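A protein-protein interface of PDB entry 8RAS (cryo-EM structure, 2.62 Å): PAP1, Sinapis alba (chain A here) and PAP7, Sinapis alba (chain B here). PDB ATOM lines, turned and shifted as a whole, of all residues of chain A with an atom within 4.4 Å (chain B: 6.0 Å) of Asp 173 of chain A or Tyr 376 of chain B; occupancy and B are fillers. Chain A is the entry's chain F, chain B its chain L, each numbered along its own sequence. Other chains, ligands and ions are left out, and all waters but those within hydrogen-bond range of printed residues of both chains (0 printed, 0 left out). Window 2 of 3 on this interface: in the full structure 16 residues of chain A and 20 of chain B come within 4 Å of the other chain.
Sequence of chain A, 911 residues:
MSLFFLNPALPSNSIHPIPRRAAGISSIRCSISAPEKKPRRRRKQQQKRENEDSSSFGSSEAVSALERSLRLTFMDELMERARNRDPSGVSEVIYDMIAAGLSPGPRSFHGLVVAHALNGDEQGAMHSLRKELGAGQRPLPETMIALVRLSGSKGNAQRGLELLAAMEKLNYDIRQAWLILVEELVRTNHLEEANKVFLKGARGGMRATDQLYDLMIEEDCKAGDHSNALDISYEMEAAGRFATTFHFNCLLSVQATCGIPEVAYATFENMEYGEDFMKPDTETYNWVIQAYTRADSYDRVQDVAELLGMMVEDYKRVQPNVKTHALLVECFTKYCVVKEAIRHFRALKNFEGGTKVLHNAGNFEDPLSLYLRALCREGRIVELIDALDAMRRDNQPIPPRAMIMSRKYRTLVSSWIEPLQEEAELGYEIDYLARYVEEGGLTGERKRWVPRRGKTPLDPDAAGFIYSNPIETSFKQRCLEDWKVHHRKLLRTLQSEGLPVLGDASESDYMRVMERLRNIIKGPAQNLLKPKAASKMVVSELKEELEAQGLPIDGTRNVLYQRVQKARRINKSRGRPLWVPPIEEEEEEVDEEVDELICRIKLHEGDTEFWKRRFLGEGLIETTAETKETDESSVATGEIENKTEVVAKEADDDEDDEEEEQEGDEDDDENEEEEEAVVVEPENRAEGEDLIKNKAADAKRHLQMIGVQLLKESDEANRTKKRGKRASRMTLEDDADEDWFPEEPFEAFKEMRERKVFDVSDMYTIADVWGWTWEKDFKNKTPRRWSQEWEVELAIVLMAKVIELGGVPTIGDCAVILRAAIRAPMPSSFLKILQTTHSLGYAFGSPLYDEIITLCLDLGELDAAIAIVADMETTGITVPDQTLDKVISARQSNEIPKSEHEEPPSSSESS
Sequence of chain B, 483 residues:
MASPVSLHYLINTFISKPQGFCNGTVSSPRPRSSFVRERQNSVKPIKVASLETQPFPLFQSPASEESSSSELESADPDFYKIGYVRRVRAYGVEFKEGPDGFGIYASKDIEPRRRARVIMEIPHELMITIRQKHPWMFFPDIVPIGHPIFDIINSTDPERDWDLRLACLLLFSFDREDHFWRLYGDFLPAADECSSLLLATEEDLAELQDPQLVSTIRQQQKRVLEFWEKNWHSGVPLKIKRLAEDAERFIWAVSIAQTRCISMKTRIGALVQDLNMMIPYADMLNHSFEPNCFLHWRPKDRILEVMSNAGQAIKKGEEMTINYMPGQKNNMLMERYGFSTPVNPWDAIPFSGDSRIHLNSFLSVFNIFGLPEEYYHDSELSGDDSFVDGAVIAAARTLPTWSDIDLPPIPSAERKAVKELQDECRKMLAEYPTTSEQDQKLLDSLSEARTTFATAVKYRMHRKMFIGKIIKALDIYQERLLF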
ATOM      1  N   TYR A 172      -0.972  12.761  34.894  1.00  0.00           N
ATOM      2  CA  TYR A 172      -1.386  12.562  33.515  1.00  0.00           C
ATOM      3  C   TYR A 172      -1.020  11.156  33.056  1.00  0.00           C
ATOM      4  O   TYR A 172      -0.067  10.550  33.552  1.00  0.00           O
ATOM      5  CB  TYR A 172      -0.736  13.592  32.585  1.00  0.00           C
ATOM      6  CG  TYR A 172      -1.482  14.900  32.492  1.00  0.00           C
ATOM      7  CD1 TYR A 172      -2.868  14.936  32.532  1.00  0.00           C
ATOM      8  CD2 TYR A 172      -0.800  16.102  32.360  1.00  0.00           C
ATOM      9  CE1 TYR A 172      -3.553  16.131  32.446  1.00  0.00           C
ATOM     10  CE2 TYR A 172      -1.477  17.301  32.273  1.00  0.00           C
ATOM     11  CZ  TYR A 172      -2.853  17.310  32.317  1.00  0.00           C
ATOM     12  OH  TYR A 172      -3.532  18.503  32.231  1.00  0.00           O
ATOM     13  N   ASP A 173      -1.792  10.644  32.100  1.00  0.00           N
ATOM     14  CA  ASP A 173      -1.523   9.338  31.505  1.00  0.00           C
ATOM     15  C   ASP A 173      -0.434   9.501  30.454  1.00  0.00           C
ATOM     16  O   ASP A 173      -0.638  10.168  29.434  1.00  0.00           O
ATOM     17  CB  ASP A 173      -2.797   8.756  30.898  1.00  0.00           C
ATOM     18  CG  ASP A 173      -2.546   7.465  30.144  1.00  0.00           C
ATOM     19  OD1 ASP A 173      -2.183   7.529  28.950  1.00  0.00           O
ATOM     20  OD2 ASP A 173      -2.716   6.383  30.744  1.00  0.00           O
ATOM     21  N   ILE A 174       0.725   8.889  30.694  1.00  0.00           N
ATOM     22  CA  ILE A 174       1.894   9.084  29.847  1.00  0.00           C
ATOM     23  C   ILE A 174       2.050   7.974  28.813  1.00  0.00           C
ATOM     24  O   ILE A 174       3.059   7.936  28.104  1.00  0.00           O
ATOM     25  CB  ILE A 174       3.170   9.220  30.691  1.00  0.00           C
ATOM     26  CG1 ILE A 174       3.552   7.872  31.303  1.00  0.00           C
ATOM     27  CG2 ILE A 174       2.977  10.257  31.780  1.00  0.00           C
ATOM     28  CD1 ILE A 174       4.866   7.895  32.046  1.00  0.00           C
ATOM     29  N   ARG A 175       1.077   7.066  28.709  1.00  0.00           N
ATOM     30  CA  ARG A 175       1.198   5.972  27.750  1.00  0.00           C
ATOM     31  C   ARG A 175       1.186   6.489  26.317  1.00  0.00           C
ATOM     32  O   ARG A 175       2.031   6.100  25.501  1.00  0.00           O
ATOM     33  CB  ARG A 175       0.080   4.952  27.961  1.00  0.00           C
ATOM     34  CG  ARG A 175      -0.048   3.953  26.820  1.00  0.00           C
ATOM     35  CD  ARG A 175      -0.821   2.715  27.233  1.00  0.00           C
ATOM     36  NE  ARG A 175      -0.621   1.617  26.295  1.00  0.00           N
ATOM     37  CZ  ARG A 175      -1.547   1.159  25.466  1.00  0.00           C
ATOM     38  NH1 ARG A 175      -2.760   1.685  25.425  1.00  0.00           N
ATOM     39  NH2 ARG A 175      -1.250   0.148  24.655  1.00  0.00           N
ATOM     40  N   GLN A 176       0.237   7.369  25.992  1.00  0.00           N
ATOM     41  CA  GLN A 176       0.147   7.888  24.631  1.00  0.00           C
ATOM     42  C   GLN A 176       1.389   8.688  24.260  1.00  0.00           C
ATOM     43  O   GLN A 176       1.916   8.552  23.149  1.00  0.00           O
ATOM     44  CB  GLN A 176      -1.109   8.743  24.480  1.00  0.00           C
ATOM     45  CG  GLN A 176      -1.541   8.958  23.041  1.00  0.00           C
ATOM     46  CD  GLN A 176      -2.956   9.488  22.932  1.00  0.00           C
ATOM     47  OE1 GLN A 176      -3.756   9.351  23.858  1.00  0.00           O
ATOM     48  NE2 GLN A 176      -3.274  10.098  21.797  1.00  0.00           N
ATOM     49  N   ASN B 367     -11.375  15.344  30.129  1.00  0.00           N
ATOM     50  CA  ASN B 367     -10.394  14.450  30.742  1.00  0.00           C
ATOM     51  C   ASN B 367     -10.659  12.994  30.353  1.00  0.00           C
ATOM     52  O   ASN B 367     -10.874  12.121  31.195  1.00  0.00           O
ATOM     53  CB  ASN B 367     -10.368  14.623  32.265  1.00  0.00           C
ATOM     54  CG  ASN B 367      -9.661  15.891  32.694  1.00  0.00           C
ATOM     55  OD1 ASN B 367      -8.717  16.339  32.044  1.00  0.00           O
ATOM     56  ND2 ASN B 367     -10.112  16.475  33.795  1.00  0.00           N
ATOM     57  N   ILE B 368     -10.642  12.749  29.047  1.00  0.00           N
ATOM     58  CA  ILE B 368     -10.794  11.412  28.486  1.00  0.00           C
ATOM     59  C   ILE B 368      -9.460  11.039  27.857  1.00  0.00           C
ATOM     60  O   ILE B 368      -9.038  11.648  26.864  1.00  0.00           O
ATOM     61  CB  ILE B 368     -11.933  11.347  27.461  1.00  0.00           C
ATOM     62  CG1 ILE B 368     -13.220  11.918  28.057  1.00  0.00           C
ATOM     63  CG2 ILE B 368     -12.152   9.915  26.997  1.00  0.00           C
ATOM     64  CD1 ILE B 368     -14.409  11.828  27.134  1.00  0.00           C
ATOM     65  N   PHE B 369      -8.794  10.041  28.425  1.00  0.00           N
ATOM     66  CA  PHE B 369      -7.463   9.639  28.003  1.00  0.00           C
ATOM     67  C   PHE B 369      -7.500   8.241  27.396  1.00  0.00           C
ATOM     68  O   PHE B 369      -8.538   7.575  27.359  1.00  0.00           O
ATOM     69  CB  PHE B 369      -6.490   9.701  29.181  1.00  0.00           C
ATOM     70  CG  PHE B 369      -6.387  11.060  29.808  1.00  0.00           C
ATOM     71  CD1 PHE B 369      -6.406  12.200  29.025  1.00  0.00           C
ATOM     72  CD2 PHE B 369      -6.275  11.195  31.180  1.00  0.00           C
ATOM     73  CE1 PHE B 369      -6.314  13.451  29.599  1.00  0.00           C
ATOM     74  CE2 PHE B 369      -6.182  12.443  31.759  1.00  0.00           C
ATOM     75  CZ  PHE B 369      -6.202  13.573  30.969  1.00  0.00           C
ATOM     76  N   GLY B 370      -6.342   7.799  26.916  1.00  0.00           N
ATOM     77  CA  GLY B 370      -6.197   6.478  26.348  1.00  0.00           C
ATOM     78  C   GLY B 370      -6.474   6.436  24.857  1.00  0.00           C
ATOM     79  O   GLY B 370      -6.911   7.405  24.233  1.00  0.00           O
ATOM     80  N   GLU B 374      -9.773   2.379  24.337  1.00  0.00           N
ATOM     81  CA  GLU B 374      -9.695   2.344  25.793  1.00  0.00           C
ATOM     82  C   GLU B 374      -9.904   3.733  26.383  1.00  0.00           C
ATOM     83  O   GLU B 374      -9.180   4.155  27.292  1.00  0.00           O
ATOM     84  CB  GLU B 374      -8.365   1.754  26.262  1.00  0.00           C
ATOM     85  CG  GLU B 374      -7.137   2.398  25.641  1.00  0.00           C
ATOM     86  CD  GLU B 374      -5.945   2.402  26.580  1.00  0.00           C
ATOM     87  OE1 GLU B 374      -6.072   2.925  27.707  1.00  0.00           O
ATOM     88  OE2 GLU B 374      -4.881   1.878  26.191  1.00  0.00           O
ATOM     89  N   TYR B 375     -10.894   4.465  25.877  1.00  0.00           N
ATOM     90  CA  TYR B 375     -11.233   5.760  26.455  1.00  0.00           C
ATOM     91  C   TYR B 375     -11.681   5.589  27.901  1.00  0.00           C
ATOM     92  O   TYR B 375     -12.473   4.698  28.216  1.00  0.00           O
ATOM     93  CB  TYR B 375     -12.343   6.429  25.645  1.00  0.00           C
ATOM     94  CG  TYR B 375     -11.910   7.019  24.324  1.00  0.00           C
ATOM     95  CD1 TYR B 375     -10.772   7.807  24.231  1.00  0.00           C
ATOM     96  CD2 TYR B 375     -12.652   6.801  23.173  1.00  0.00           C
ATOM     97  CE1 TYR B 375     -10.381   8.351  23.023  1.00  0.00           C
ATOM     98  CE2 TYR B 375     -12.271   7.342  21.964  1.00  0.00           C
ATOM     99  CZ  TYR B 375     -11.135   8.116  21.894  1.00  0.00           C
ATOM    100  OH  TYR B 375     -10.753   8.654  20.687  1.00  0.00           O
ATOM    101  N   TYR B 376     -11.176   6.449  28.782  1.00  0.00           N
ATOM    102  CA  TYR B 376     -11.561   6.392  30.184  1.00  0.00           C
ATOM    103  C   TYR B 376     -11.429   7.775  30.805  1.00  0.00           C
ATOM    104  O   TYR B 376     -10.715   8.644  30.297  1.00  0.00           O
ATOM    105  CB  TYR B 376     -10.725   5.366  30.960  1.00  0.00           C
ATOM    106  CG  TYR B 376      -9.268   5.729  31.124  1.00  0.00           C
ATOM    107  CD1 TYR B 376      -8.365   5.550  30.084  1.00  0.00           C
ATOM    108  CD2 TYR B 376      -8.790   6.237  32.324  1.00  0.00           C
ATOM    109  CE1 TYR B 376      -7.033   5.874  30.233  1.00  0.00           C
ATOM    110  CE2 TYR B 376      -7.460   6.565  32.482  1.00  0.00           C
ATOM    111  CZ  TYR B 376      -6.584   6.381  31.434  1.00  0.00           C
ATOM    112  OH  TYR B 376      -5.258   6.707  31.587  1.00  0.00           O
ATOM    113  N   HIS B 377     -12.131   7.964  31.917  1.00  0.00           N
ATOM    114  CA  HIS B 377     -12.201   9.238  32.616  1.00  0.00           C
ATOM    115  C   HIS B 377     -11.376   9.167  33.893  1.00  0.00           C
ATOM    116  O   HIS B 377     -11.392   8.154  34.597  1.00  0.00           O
ATOM    117  CB  HIS B 377     -13.656   9.589  32.942  1.00  0.00           C
ATOM    118  CG  HIS B 377     -13.816  10.846  33.739  1.00  0.00           C
ATOM    119  ND1 HIS B 377     -13.217  12.034  33.383  1.00  0.00           N
ATOM    120  CD2 HIS B 377     -14.514  11.100  34.871  1.00  0.00           C
ATOM    121  CE1 HIS B 377     -13.538  12.967  34.262  1.00  0.00           C
ATOM    122  NE2 HIS B 377     -14.323  12.426  35.175  1.00  0.00           N
ATOM    123  N   ASP B 378     -10.651  10.244  34.185  1.00  0.00           N
ATOM    124  CA  ASP B 378      -9.748  10.270  35.335  1.00  0.00           C
ATOM    125  C   ASP B 378     -10.494  10.178  36.668  1.00  0.00           C
ATOM    126  O   ASP B 378     -11.718  10.284  36.718  1.00  0.00           O
ATOM    127  CB  ASP B 378      -8.879  11.534  35.304  1.00  0.00           C
ATOM    128  CG  ASP B 378      -9.629  12.783  35.748  1.00  0.00           C
ATOM    129  OD1 ASP B 378     -10.868  12.832  35.603  1.00  0.00           O
ATOM    130  OD2 ASP B 378      -8.973  13.721  36.247  1.00  0.00           O
ATOM    131  N   ILE B 393     -18.042   9.517  26.632  1.00  0.00           N
ATOM    132  CA  ILE B 393     -17.143   8.656  25.869  1.00  0.00           C
ATOM    133  C   ILE B 393     -17.810   8.195  24.579  1.00  0.00           C
ATOM    134  O   ILE B 393     -17.184   8.172  23.511  1.00  0.00           O
ATOM    135  CB  ILE B 393     -16.692   7.465  26.734  1.00  0.00           C
ATOM    136  CG1 ILE B 393     -15.844   7.954  27.908  1.00  0.00           C
ATOM    137  CG2 ILE B 393     -15.930   6.454  25.899  1.00  0.00           C
ATOM    138  CD1 ILE B 393     -15.752   6.966  29.042  1.00  0.00           C
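The side-chain hydroxyl (OH) of Tyr 376 of chain B lies within hydrogen-bond range of the side-chain carboxylate (OD2) of Asp 173 of chain A (2.7 Å).
OE2 of Glu 374 of chain B sits close to NH1 of Arg 175 of chain A (2.3 Å).
The backbone NH of Arg 175 of chain A lies within hydrogen-bond range of the side-chain carboxylate of Asp 173 of chain A (3.3 Å).
The backbone NH (N) of Phe 369 of chain B lies within hydrogen-bond range of the backbone carbonyl oxygen (O) of Tyr 376 of chain B, 3.0 Å away.
Tyr 172 of chain A touches Phe 369 of chain B (CD1 to CZ, 3.9 Å).
Gly 370 of chain B touches Gln 176 of chain A.
Printed residues of chain B within 4 Å of Tyr 172 of chain A: Phe 369 (3.9 Å).
Of chain B, only Tyr 376 comes within 4 Å of Asp 173 of chain A.
Of the printed residues of chain B, Arg 175 of chain A touches Glu 374.
Of the printed residues of chain B, Gln 176 of chain A touches Gly 370.
Printed residues of chain A within 4 Å of Phe 369 of chain B: Tyr 172.
Of the printed residues of chain A, Gly 370 of chain B touches Gln 176 (3.7 Å).
Printed residues of chain A within 4 Å of Tyr 376 of chain B: Asp 173.
Asp 378 of chain B touches none of the printed residues of chain A.
Ile 393 of chain B touches none of the printed residues of chain A.
The nearest residue of chain B that does not touch Asp 173 of chain A is Phe 369 of chain B (4.2 Å).
Printed residues of chain A that touch a printed residue of chain B: Tyr 172, Asp 173, Arg 175 and Gln 176.
Of the 10 printed residues of chain B, 4 touch a printed residue of chain A.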
